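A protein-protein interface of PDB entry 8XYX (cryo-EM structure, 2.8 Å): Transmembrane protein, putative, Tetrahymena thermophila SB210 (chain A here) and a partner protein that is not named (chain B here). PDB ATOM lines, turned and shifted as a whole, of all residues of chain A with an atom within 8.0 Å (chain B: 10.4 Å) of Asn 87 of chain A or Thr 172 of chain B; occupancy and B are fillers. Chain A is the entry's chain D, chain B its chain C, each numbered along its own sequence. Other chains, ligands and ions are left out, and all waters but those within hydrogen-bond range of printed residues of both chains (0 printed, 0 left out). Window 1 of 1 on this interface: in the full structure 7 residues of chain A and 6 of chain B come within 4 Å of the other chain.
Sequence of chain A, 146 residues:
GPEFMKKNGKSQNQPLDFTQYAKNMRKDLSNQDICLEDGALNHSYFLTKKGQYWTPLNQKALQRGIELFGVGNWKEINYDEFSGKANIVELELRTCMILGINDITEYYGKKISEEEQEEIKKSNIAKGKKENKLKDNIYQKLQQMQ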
ATOM      1  N   GLN A  52      15.509 -18.066 -11.343  1.00  0.00           N
ATOM      2  CA  GLN A  52      14.436 -18.709 -12.102  1.00  0.00           C
ATOM      3  C   GLN A  52      13.203 -18.770 -11.205  1.00  0.00           C
ATOM      4  O   GLN A  52      13.035 -19.718 -10.434  1.00  0.00           O
ATOM      5  CB  GLN A  52      14.859 -20.095 -12.578  1.00  0.00           C
ATOM      6  CG  GLN A  52      15.921 -20.751 -11.711  1.00  0.00           C
ATOM      7  CD  GLN A  52      16.493 -22.007 -12.338  1.00  0.00           C
ATOM      8  OE1 GLN A  52      15.898 -22.588 -13.243  1.00  0.00           O
ATOM      9  NE2 GLN A  52      17.654 -22.434 -11.855  1.00  0.00           N
ATOM     10  N   TRP A  54       9.858 -17.110 -12.532  1.00  0.00           N
ATOM     11  CA  TRP A  54       8.666 -16.930 -13.366  1.00  0.00           C
ATOM     12  C   TRP A  54       7.611 -16.087 -12.643  1.00  0.00           C
ATOM     13  O   TRP A  54       6.576 -16.576 -12.183  1.00  0.00           O
ATOM     14  CB  TRP A  54       8.076 -18.263 -13.835  1.00  0.00           C
ATOM     15  CG  TRP A  54       7.052 -18.068 -14.886  1.00  0.00           C
ATOM     16  CD1 TRP A  54       5.702 -18.164 -14.743  1.00  0.00           C
ATOM     17  CD2 TRP A  54       7.289 -17.714 -16.248  1.00  0.00           C
ATOM     18  NE1 TRP A  54       5.082 -17.905 -15.938  1.00  0.00           N
ATOM     19  CE2 TRP A  54       6.036 -17.625 -16.879  1.00  0.00           C
ATOM     20  CE3 TRP A  54       8.441 -17.470 -16.998  1.00  0.00           C
ATOM     21  CZ2 TRP A  54       5.901 -17.303 -18.222  1.00  0.00           C
ATOM     22  CZ3 TRP A  54       8.307 -17.151 -18.327  1.00  0.00           C
ATOM     23  CH2 TRP A  54       7.047 -17.073 -18.929  1.00  0.00           C
ATOM     24  N   TRP A  74       9.353 -18.298 -30.288  1.00  0.00           N
ATOM     25  CA  TRP A  74       9.834 -17.918 -28.966  1.00  0.00           C
ATOM     26  C   TRP A  74      10.990 -16.930 -29.024  1.00  0.00           C
ATOM     27  O   TRP A  74      11.225 -16.219 -28.044  1.00  0.00           O
ATOM     28  CB  TRP A  74      10.266 -19.154 -28.177  1.00  0.00           C
ATOM     29  CG  TRP A  74       9.329 -20.322 -28.275  1.00  0.00           C
ATOM     30  CD1 TRP A  74       9.626 -21.568 -28.745  1.00  0.00           C
ATOM     31  CD2 TRP A  74       7.952 -20.363 -27.876  1.00  0.00           C
ATOM     32  NE1 TRP A  74       8.521 -22.379 -28.672  1.00  0.00           N
ATOM     33  CE2 TRP A  74       7.480 -21.663 -28.143  1.00  0.00           C
ATOM     34  CE3 TRP A  74       7.072 -19.426 -27.325  1.00  0.00           C
ATOM     35  CZ2 TRP A  74       6.170 -22.049 -27.878  1.00  0.00           C
ATOM     36  CZ3 TRP A  74       5.772 -19.812 -27.064  1.00  0.00           C
ATOM     37  CH2 TRP A  74       5.334 -21.111 -27.341  1.00  0.00           C
ATOM     38  N   ASN A  78      11.423 -13.682 -26.679  1.00  0.00           N
ATOM     39  CA  ASN A  78      12.634 -13.524 -25.880  1.00  0.00           C
ATOM     40  C   ASN A  78      13.313 -12.189 -26.158  1.00  0.00           C
ATOM     41  O   ASN A  78      13.799 -11.526 -25.235  1.00  0.00           O
ATOM     42  CB  ASN A  78      13.595 -14.678 -26.166  1.00  0.00           C
ATOM     43  CG  ASN A  78      14.582 -14.916 -25.040  1.00  0.00           C
ATOM     44  OD1 ASN A  78      14.994 -13.988 -24.345  1.00  0.00           O
ATOM     45  ND2 ASN A  78      14.976 -16.170 -24.862  1.00  0.00           N
ATOM     46  N   PHE A  82      10.176  -9.982 -23.144  1.00  0.00           N
ATOM     47  CA  PHE A  82      10.723 -10.253 -21.821  1.00  0.00           C
ATOM     48  C   PHE A  82      11.916  -9.364 -21.501  1.00  0.00           C
ATOM     49  O   PHE A  82      11.832  -8.534 -20.588  1.00  0.00           O
ATOM     50  CB  PHE A  82      11.124 -11.730 -21.717  1.00  0.00           C
ATOM     51  CG  PHE A  82       9.982 -12.643 -21.396  1.00  0.00           C
ATOM     52  CD1 PHE A  82       9.592 -12.849 -20.085  1.00  0.00           C
ATOM     53  CD2 PHE A  82       9.294 -13.290 -22.407  1.00  0.00           C
ATOM     54  CE1 PHE A  82       8.537 -13.684 -19.788  1.00  0.00           C
ATOM     55  CE2 PHE A  82       8.239 -14.126 -22.116  1.00  0.00           C
ATOM     56  CZ  PHE A  82       7.861 -14.322 -20.806  1.00  0.00           C
ATOM     57  N   GLY A  84      16.301 -10.008 -22.605  1.00  0.00           N
ATOM     58  CA  GLY A  84      17.231 -10.754 -23.426  1.00  0.00           C
ATOM     59  C   GLY A  84      17.606 -12.046 -22.732  1.00  0.00           C
ATOM     60  O   GLY A  84      18.432 -12.819 -23.227  1.00  0.00           O
ATOM     61  N   LYS A  85      16.994 -12.285 -21.573  1.00  0.00           N
ATOM     62  CA  LYS A  85      17.269 -13.454 -20.741  1.00  0.00           C
ATOM     63  C   LYS A  85      15.958 -14.200 -20.516  1.00  0.00           C
ATOM     64  O   LYS A  85      15.171 -13.833 -19.637  1.00  0.00           O
ATOM     65  CB  LYS A  85      17.900 -13.043 -19.413  1.00  0.00           C
ATOM     66  CG  LYS A  85      19.326 -12.533 -19.523  1.00  0.00           C
ATOM     67  CD  LYS A  85      19.888 -12.199 -18.150  1.00  0.00           C
ATOM     68  CE  LYS A  85      21.334 -11.738 -18.236  1.00  0.00           C
ATOM     69  NZ  LYS A  85      21.882 -11.396 -16.893  1.00  0.00           N
ATOM     70  N   ALA A  86      15.728 -15.249 -21.303  1.00  0.00           N
ATOM     71  CA  ALA A  86      14.538 -16.082 -21.148  1.00  0.00           C
ATOM     72  C   ALA A  86      14.821 -17.432 -21.781  1.00  0.00           C
ATOM     73  O   ALA A  86      15.213 -17.495 -22.950  1.00  0.00           O
ATOM     74  CB  ALA A  86      13.316 -15.427 -21.791  1.00  0.00           C
ATOM     75  N   ASN A  87      14.633 -18.505 -21.018  1.00  0.00           N
ATOM     76  CA  ASN A  87      14.828 -19.848 -21.547  1.00  0.00           C
ATOM     77  C   ASN A  87      13.727 -20.167 -22.549  1.00  0.00           C
ATOM     78  O   ASN A  87      12.540 -20.059 -22.231  1.00  0.00           O
ATOM     79  CB  ASN A  87      14.830 -20.869 -20.413  1.00  0.00           C
ATOM     80  CG  ASN A  87      16.212 -21.399 -20.109  1.00  0.00           C
ATOM     81  OD1 ASN A  87      17.216 -20.751 -20.402  1.00  0.00           O
ATOM     82  ND2 ASN A  87      16.273 -22.586 -19.521  1.00  0.00           N
ATOM     83  N   ILE A  88      14.125 -20.557 -23.763  1.00  0.00           N
ATOM     84  CA  ILE A  88      13.153 -20.945 -24.782  1.00  0.00           C
ATOM     85  C   ILE A  88      12.401 -22.195 -24.347  1.00  0.00           C
ATOM     86  O   ILE A  88      11.192 -22.331 -24.583  1.00  0.00           O
ATOM     87  CB  ILE A  88      13.862 -21.143 -26.135  1.00  0.00           C
ATOM     88  CG1 ILE A  88      14.588 -19.861 -26.547  1.00  0.00           C
ATOM     89  CG2 ILE A  88      12.877 -21.564 -27.213  1.00  0.00           C
ATOM     90  CD1 ILE A  88      13.672 -18.673 -26.732  1.00  0.00           C
ATOM     91  N   VAL A  89      13.103 -23.117 -23.685  1.00  0.00           N
ATOM     92  CA  VAL A  89      12.472 -24.329 -23.168  1.00  0.00           C
ATOM     93  C   VAL A  89      11.416 -23.975 -22.129  1.00  0.00           C
ATOM     94  O   VAL A  89      10.298 -24.507 -22.147  1.00  0.00           O
ATOM     95  CB  VAL A  89      13.541 -25.276 -22.593  1.00  0.00           C
ATOM     96  CG1 VAL A  89      12.902 -26.389 -21.778  1.00  0.00           C
ATOM     97  CG2 VAL A  89      14.401 -25.842 -23.710  1.00  0.00           C
ATOM     98  N   GLU A  90      11.745 -23.053 -21.221  1.00  0.00           N
ATOM     99  CA  GLU A  90      10.787 -22.658 -20.193  1.00  0.00           C
ATOM    100  C   GLU A  90       9.610 -21.898 -20.791  1.00  0.00           C
ATOM    101  O   GLU A  90       8.477 -22.057 -20.332  1.00  0.00           O
ATOM    102  CB  GLU A  90      11.470 -21.820 -19.114  1.00  0.00           C
ATOM    103  CG  GLU A  90      10.744 -21.863 -17.780  1.00  0.00           C
ATOM    104  CD  GLU A  90      11.221 -20.799 -16.815  1.00  0.00           C
ATOM    105  OE1 GLU A  90      12.054 -19.959 -17.215  1.00  0.00           O
ATOM    106  OE2 GLU A  90      10.762 -20.803 -15.652  1.00  0.00           O
ATOM    107  N   LEU A  91       9.857 -21.064 -21.806  1.00  0.00           N
ATOM    108  CA  LEU A  91       8.755 -20.379 -22.476  1.00  0.00           C
ATOM    109  C   LEU A  91       7.813 -21.373 -23.139  1.00  0.00           C
ATOM    110  O   LEU A  91       6.587 -21.239 -23.034  1.00  0.00           O
ATOM    111  CB  LEU A  91       9.288 -19.387 -23.510  1.00  0.00           C
ATOM    112  CG  LEU A  91       9.989 -18.116 -23.025  1.00  0.00           C
ATOM    113  CD1 LEU A  91       9.776 -16.989 -24.020  1.00  0.00           C
ATOM    114  CD2 LEU A  91       9.504 -17.705 -21.649  1.00  0.00           C
ATOM    115  N   GLU A  92       8.369 -22.391 -23.802  1.00  0.00           N
ATOM    116  CA  GLU A  92       7.542 -23.430 -24.410  1.00  0.00           C
ATOM    117  C   GLU A  92       6.747 -24.193 -23.357  1.00  0.00           C
ATOM    118  O   GLU A  92       5.556 -24.465 -23.549  1.00  0.00           O
ATOM    119  CB  GLU A  92       8.418 -24.383 -25.224  1.00  0.00           C
ATOM    120  CG  GLU A  92       7.877 -25.803 -25.339  1.00  0.00           C
ATOM    121  CD  GLU A  92       8.666 -26.655 -26.314  1.00  0.00           C
ATOM    122  OE1 GLU A  92       9.631 -26.138 -26.913  1.00  0.00           O
ATOM    123  OE2 GLU A  92       8.318 -27.843 -26.481  1.00  0.00           O
ATOM    124  N   LEU A  93       7.381 -24.527 -22.228  1.00  0.00           N
ATOM    125  CA  LEU A  93       6.695 -25.283 -21.182  1.00  0.00           C
ATOM    126  C   LEU A  93       5.569 -24.474 -20.542  1.00  0.00           C
ATOM    127  O   LEU A  93       4.463 -24.992 -20.339  1.00  0.00           O
ATOM    128  CB  LEU A  93       7.701 -25.735 -20.125  1.00  0.00           C
ATOM    129  CG  LEU A  93       8.653 -26.854 -20.554  1.00  0.00           C
ATOM    130  CD1 LEU A  93       9.597 -27.231 -19.427  1.00  0.00           C
ATOM    131  CD2 LEU A  93       7.869 -28.063 -21.021  1.00  0.00           C
ATOM    132  N   ARG A  94       5.826 -23.201 -20.226  1.00  0.00           N
ATOM    133  CA  ARG A  94       4.791 -22.358 -19.635  1.00  0.00           C
ATOM    134  C   ARG A  94       3.650 -22.111 -20.615  1.00  0.00           C
ATOM    135  O   ARG A  94       2.475 -22.131 -20.223  1.00  0.00           O
ATOM    136  CB  ARG A  94       5.388 -21.032 -19.163  1.00  0.00           C
ATOM    137  CG  ARG A  94       6.461 -21.166 -18.091  1.00  0.00           C
ATOM    138  CD  ARG A  94       5.890 -21.358 -16.701  1.00  0.00           C
ATOM    139  NE  ARG A  94       6.952 -21.456 -15.706  1.00  0.00           N
ATOM    140  CZ  ARG A  94       6.763 -21.773 -14.434  1.00  0.00           C
ATOM    141  NH1 ARG A  94       5.556 -22.022 -13.955  1.00  0.00           N
ATOM    142  NH2 ARG A  94       7.812 -21.843 -13.621  1.00  0.00           N
ATOM    143  N   ILE B 160      23.525 -35.957 -17.339  1.00  0.00           N
ATOM    144  CA  ILE B 160      22.398 -35.043 -17.174  1.00  0.00           C
ATOM    145  C   ILE B 160      21.565 -35.430 -15.958  1.00  0.00           C
ATOM    146  O   ILE B 160      21.194 -34.579 -15.141  1.00  0.00           O
ATOM    147  CB  ILE B 160      21.547 -35.016 -18.456  1.00  0.00           C
ATOM    148  CG1 ILE B 160      22.385 -34.530 -19.638  1.00  0.00           C
ATOM    149  CG2 ILE B 160      20.327 -34.139 -18.270  1.00  0.00           C
ATOM    150  CD1 ILE B 160      21.733 -34.760 -20.975  1.00  0.00           C
ATOM    151  N   PHE B 165      20.425 -31.272  -9.974  1.00  0.00           N
ATOM    152  CA  PHE B 165      19.921 -30.374 -10.999  1.00  0.00           C
ATOM    153  C   PHE B 165      18.408 -30.262 -10.889  1.00  0.00           C
ATOM    154  O   PHE B 165      17.720 -31.229 -10.548  1.00  0.00           O
ATOM    155  CB  PHE B 165      20.297 -30.869 -12.400  1.00  0.00           C
ATOM    156  CG  PHE B 165      21.614 -30.351 -12.900  1.00  0.00           C
ATOM    157  CD1 PHE B 165      22.525 -29.773 -12.031  1.00  0.00           C
ATOM    158  CD2 PHE B 165      21.944 -30.449 -14.242  1.00  0.00           C
ATOM    159  CE1 PHE B 165      23.738 -29.298 -12.492  1.00  0.00           C
ATOM    160  CE2 PHE B 165      23.154 -29.978 -14.709  1.00  0.00           C
ATOM    161  CZ  PHE B 165      24.052 -29.401 -13.832  1.00  0.00           C
ATOM    162  N   THR B 166      17.895 -29.072 -11.183  1.00  0.00           N
ATOM    163  CA  THR B 166      16.456 -28.870 -11.218  1.00  0.00           C
ATOM    164  C   THR B 166      15.859 -29.533 -12.455  1.00  0.00           C
ATOM    165  O   THR B 166      16.564 -29.892 -13.402  1.00  0.00           O
ATOM    166  CB  THR B 166      16.117 -27.381 -11.214  1.00  0.00           C
ATOM    167  OG1 THR B 166      16.067 -26.901 -12.563  1.00  0.00           O
ATOM    168  CG2 THR B 166      17.165 -26.597 -10.442  1.00  0.00           C
ATOM    169  N   ASN B 167      14.533 -29.701 -12.432  1.00  0.00           N
ATOM    170  CA  ASN B 167      13.843 -30.291 -13.575  1.00  0.00           C
ATOM    171  C   ASN B 167      13.938 -29.405 -14.810  1.00  0.00           C
ATOM    172  O   ASN B 167      13.992 -29.917 -15.932  1.00  0.00           O
ATOM    173  CB  ASN B 167      12.380 -30.558 -13.229  1.00  0.00           C
ATOM    174  CG  ASN B 167      12.223 -31.475 -12.034  1.00  0.00           C
ATOM    175  OD1 ASN B 167      13.205 -31.855 -11.398  1.00  0.00           O
ATOM    176  ND2 ASN B 167      10.985 -31.834 -11.723  1.00  0.00           N
ATOM    177  N   LEU B 168      13.962 -28.083 -14.625  1.00  0.00           N
ATOM    178  CA  LEU B 168      14.118 -27.181 -15.761  1.00  0.00           C
ATOM    179  C   LEU B 168      15.510 -27.291 -16.373  1.00  0.00           C
ATOM    180  O   LEU B 168      15.655 -27.272 -17.600  1.00  0.00           O
ATOM    181  CB  LEU B 168      13.829 -25.744 -15.338  1.00  0.00           C
ATOM    182  CG  LEU B 168      13.779 -24.739 -16.490  1.00  0.00           C
ATOM    183  CD1 LEU B 168      12.630 -25.063 -17.428  1.00  0.00           C
ATOM    184  CD2 LEU B 168      13.670 -23.318 -15.965  1.00  0.00           C
ATOM    185  N   GLU B 169      16.546 -27.403 -15.537  1.00  0.00           N
ATOM    186  CA  GLU B 169      17.901 -27.577 -16.054  1.00  0.00           C
ATOM    187  C   GLU B 169      18.051 -28.908 -16.780  1.00  0.00           C
ATOM    188  O   GLU B 169      18.682 -28.976 -17.844  1.00  0.00           O
ATOM    189  CB  GLU B 169      18.913 -27.474 -14.913  1.00  0.00           C
ATOM    190  CG  GLU B 169      19.241 -26.050 -14.495  1.00  0.00           C
ATOM    191  CD  GLU B 169      19.825 -25.980 -13.097  1.00  0.00           C
ATOM    192  OE1 GLU B 169      19.875 -27.028 -12.420  1.00  0.00           O
ATOM    193  OE2 GLU B 169      20.230 -24.877 -12.674  1.00  0.00           O
ATOM    194  N   ILE B 170      17.473 -29.975 -16.219  1.00  0.00           N
ATOM    195  CA  ILE B 170      17.506 -31.283 -16.867  1.00  0.00           C
ATOM    196  C   ILE B 170      16.777 -31.232 -18.202  1.00  0.00           C
ATOM    197  O   ILE B 170      17.264 -31.761 -19.208  1.00  0.00           O
ATOM    198  CB  ILE B 170      16.915 -32.356 -15.932  1.00  0.00           C
ATOM    199  CG1 ILE B 170      17.834 -32.586 -14.733  1.00  0.00           C
ATOM    200  CG2 ILE B 170      16.687 -33.663 -16.674  1.00  0.00           C
ATOM    201  CD1 ILE B 170      17.171 -33.316 -13.588  1.00  0.00           C
ATOM    202  N   LEU B 171      15.615 -30.574 -18.239  1.00  0.00           N
ATOM    203  CA  LEU B 171      14.860 -30.460 -19.484  1.00  0.00           C
ATOM    204  C   LEU B 171      15.611 -29.634 -20.521  1.00  0.00           C
ATOM    205  O   LEU B 171      15.571 -29.946 -21.715  1.00  0.00           O
ATOM    206  CB  LEU B 171      13.484 -29.857 -19.213  1.00  0.00           C
ATOM    207  CG  LEU B 171      12.306 -30.828 -19.286  1.00  0.00           C
ATOM    208  CD1 LEU B 171      11.579 -30.905 -17.952  1.00  0.00           C
ATOM    209  CD2 LEU B 171      11.356 -30.423 -20.398  1.00  0.00           C
ATOM    210  N   THR B 172      16.297 -28.574 -20.086  1.00  0.00           N
ATOM    211  CA  THR B 172      17.085 -27.767 -21.013  1.00  0.00           C
ATOM    212  C   THR B 172      18.242 -28.569 -21.597  1.00  0.00           C
ATOM    213  O   THR B 172      18.504 -28.506 -22.806  1.00  0.00           O
ATOM    214  CB  THR B 172      17.602 -26.513 -20.307  1.00  0.00           C
ATOM    215  OG1 THR B 172      16.495 -25.754 -19.807  1.00  0.00           O
ATOM    216  CG2 THR B 172      18.400 -25.644 -21.267  1.00  0.00           C
ATOM    217  N   HIS B 173      18.937 -29.341 -20.755  1.00  0.00           N
ATOM    218  CA  HIS B 173      20.019 -30.190 -21.247  1.00  0.00           C
ATOM    219  C   HIS B 173      19.498 -31.253 -22.206  1.00  0.00           C
ATOM    220  O   HIS B 173      20.125 -31.534 -23.235  1.00  0.00           O
ATOM    221  CB  HIS B 173      20.750 -30.843 -20.074  1.00  0.00           C
ATOM    222  CG  HIS B 173      21.579 -29.890 -19.273  1.00  0.00           C
ATOM    223  ND1 HIS B 173      22.235 -28.818 -19.838  1.00  0.00           N
ATOM    224  CD2 HIS B 173      21.863 -29.850 -17.950  1.00  0.00           C
ATOM    225  CE1 HIS B 173      22.884 -28.156 -18.897  1.00  0.00           C
ATOM    226  NE2 HIS B 173      22.676 -28.762 -17.743  1.00  0.00           N
ATOM    227  N   LEU B 174      18.346 -31.849 -21.887  1.00  0.00           N
ATOM    228  CA  LEU B 174      17.757 -32.860 -22.759  1.00  0.00           C
ATOM    229  C   LEU B 174      17.339 -32.266 -24.098  1.00  0.00           C
ATOM    230  O   LEU B 174      17.530 -32.891 -25.148  1.00  0.00           O
ATOM    231  CB  LEU B 174      16.561 -33.505 -22.062  1.00  0.00           C
ATOM    232  CG  LEU B 174      16.816 -34.433 -20.871  1.00  0.00           C
ATOM    233  CD1 LEU B 174      15.606 -35.308 -20.599  1.00  0.00           C
ATOM    234  CD2 LEU B 174      18.056 -35.281 -21.084  1.00  0.00           C
ATOM    235  N   TYR B 175      16.768 -31.059 -24.084  1.00  0.00           N
ATOM    236  CA  TYR B 175      16.370 -30.409 -25.328  1.00  0.00           C
ATOM    237  C   TYR B 175      17.582 -30.027 -26.167  1.00  0.00           C
ATOM    238  O   TYR B 175      17.552 -30.147 -27.398  1.00  0.00           O
ATOM    239  CB  TYR B 175      15.511 -29.181 -25.029  1.00  0.00           C
ATOM    240  CG  TYR B 175      14.025 -29.459 -25.046  1.00  0.00           C
ATOM    241  CD1 TYR B 175      13.361 -29.712 -26.239  1.00  0.00           C
ATOM    242  CD2 TYR B 175      13.287 -29.470 -23.870  1.00  0.00           C
ATOM    243  CE1 TYR B 175      12.003 -29.967 -26.261  1.00  0.00           C
ATOM    244  CE2 TYR B 175      11.930 -29.725 -23.882  1.00  0.00           C
ATOM    245  CZ  TYR B 175      11.295 -29.973 -25.079  1.00  0.00           C
ATOM    246  OH  TYR B 175       9.943 -30.226 -25.093  1.00  0.00           O
ATOM    247  N   ASN B 176      18.658 -29.563 -25.521  1.00  0.00           N
ATOM    248  CA  ASN B 176      19.887 -29.269 -26.254  1.00  0.00           C
ATOM    249  C   ASN B 176      20.478 -30.530 -26.872  1.00  0.00           C
ATOM    250  O   ASN B 176      20.947 -30.508 -28.017  1.00  0.00           O
ATOM    251  CB  ASN B 176      20.901 -28.595 -25.331  1.00  0.00           C
ATOM    252  CG  ASN B 176      20.870 -27.083 -25.438  1.00  0.00           C
ATOM    253  OD1 ASN B 176      20.303 -26.527 -26.379  1.00  0.00           O
ATOM    254  ND2 ASN B 176      21.482 -26.409 -24.473  1.00  0.00           N
ATOM    255  N   LEU B 177      20.459 -31.642 -26.130  1.00  0.00           N
ATOM    256  CA  LEU B 177      20.944 -32.909 -26.671  1.00  0.00           C
ATOM    257  C   LEU B 177      20.094 -33.371 -27.850  1.00  0.00           C
ATOM    258  O   LEU B 177      20.628 -33.858 -28.852  1.00  0.00           O
ATOM    259  CB  LEU B 177      20.967 -33.971 -25.572  1.00  0.00           C
ATOM    260  CG  LEU B 177      21.801 -35.233 -25.813  1.00  0.00           C
ATOM    261  CD1 LEU B 177      22.484 -35.655 -24.527  1.00  0.00           C
ATOM    262  CD2 LEU B 177      20.949 -36.373 -26.353  1.00  0.00           C
ATOM    263  N   LYS B 178      18.769 -33.233 -27.741  1.00  0.00           N
ATOM    264  CA  LYS B 178      17.884 -33.615 -28.838  1.00  0.00           C
ATOM    265  C   LYS B 178      18.131 -32.756 -30.072  1.00  0.00           C
ATOM    266  O   LYS B 178      18.160 -33.267 -31.199  1.00  0.00           O
ATOM    267  CB  LYS B 178      16.424 -33.507 -28.395  1.00  0.00           C
ATOM    268  CG  LYS B 178      15.422 -33.481 -29.540  1.00  0.00           C
ATOM    269  CD  LYS B 178      14.001 -33.675 -29.046  1.00  0.00           C
ATOM    270  CE  LYS B 178      13.001 -33.512 -30.179  1.00  0.00           C
ATOM    271  NZ  LYS B 178      12.979 -32.119 -30.701  1.00  0.00           N
ATOM    272  N   ALA B 179      18.323 -31.448 -29.877  1.00  0.00           N
ATOM    273  CA  ALA B 179      18.623 -30.562 -30.996  1.00  0.00           C
ATOM    274  C   ALA B 179      19.952 -30.923 -31.646  1.00  0.00           C
ATOM    275  O   ALA B 179      20.073 -30.905 -32.876  1.00  0.00           O
ATOM    276  CB  ALA B 179      18.634 -29.108 -30.526  1.00  0.00           C
ATOM    277  N   GLU B 180      20.959 -31.258 -30.833  1.00  0.00           N
ATOM    278  CA  GLU B 180      22.255 -31.652 -31.379  1.00  0.00           C
ATOM    279  C   GLU B 180      22.150 -32.949 -32.174  1.00  0.00           C
ATOM    280  O   GLU B 180      22.750 -33.076 -33.247  1.00  0.00           O
ATOM    281  CB  GLU B 180      23.276 -31.796 -30.251  1.00  0.00           C
ATOM    282  CG  GLU B 180      24.676 -31.288 -30.583  1.00  0.00           C
ATOM    283  CD  GLU B 180      24.732 -29.782 -30.796  1.00  0.00           C
ATOM    284  OE1 GLU B 180      25.149 -29.071 -29.858  1.00  0.00           O
ATOM    285  OE2 GLU B 180      24.387 -29.311 -31.900  1.00  0.00           O
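OG1 of Thr 172 of chain B lies within hydrogen-bond range of ND2 of Asn 87 of chain A, at 3.2 Å.
OH of Tyr 175 of chain B is in hydrogen-bond range of OE2 of Glu 92 of chain A (3.2 Å).
The backbone NH (N) of Leu 168 of chain B is in hydrogen-bond range of the side-chain hydroxyl (OG1) of Thr 166 of chain B (3.2 Å).
The backbone carbonyl oxygen of Leu 168 of chain B lies within hydrogen-bond range of the side-chain hydroxyl of Thr 172 of chain B (2.8 Å).
The side-chain hydroxyl (OG1) of Thr 166 of chain B is in hydrogen-bond range of the backbone NH (N) of Glu 169 of chain B, at 3.1 Å.
The guanidinium group (NH2) of Arg 94 of chain A is in salt-bridge range of the side-chain carboxylate (OE2) of Glu 90 of chain A.
Among the printed residues, merely in contact across the chains: Gln 52 of chain A with Leu 168 of chain B, Glu 90 of chain A with Leu 168 of chain B, Gln 52 of chain A with Glu 169 of chain B, Val 89 of chain A with Tyr 175 of chain B and Leu 93 of chain A with Leu 171 of chain B.
Asn 87 of chain A touches just one residue of chain B: Thr 172 (3.2 Å).
Thr 172 of chain B touches just one residue of chain A: Asn 87.
No residue of chain B comes within 4 Å of Ala 86 of chain A.
No residue of chain B comes within 4 Å of Ile 88 of chain A.
No residue of chain B comes within 4 Å of Leu 91 of chain A.
Of the printed residues of chain B, Leu 93 of chain A touches Leu 171 (3.8 Å).
Of the printed residues of chain B, Glu 92 of chain A touches Tyr 175.
Of the printed residues of chain A, Tyr 175 of chain B touches Val 89 (3.7 Å) and Glu 92 (3.2 Å).
The nearest residue of chain B that does not touch Asn 87 of chain A is Leu 168 of chain B (4.5 Å).
The nearest printed residue of chain A that does not touch Leu 168 of chain B is Leu 93 of chain A (4.2 Å).
Of the 17 printed residues of chain B, 5 touch a printed residue of chain A.
Hydrophobic or aromatic side chains of chain B within 4 Å of the printed part of chain A: Leu 168, Leu 171 and Tyr 175.
Of the 16 printed residues of chain A, 6 touch a printed residue of chain B.
Hydrophobic or aromatic side chains of chain A that line the printed part of chain B: Val 89 and Leu 93.
Among the printed residues, 7 pairs touch across the chains.
Among the printed residues, no Asp or Glu carboxylate lies within 4 Å of a Lys or Arg side-chain nitrogen of the other chain.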
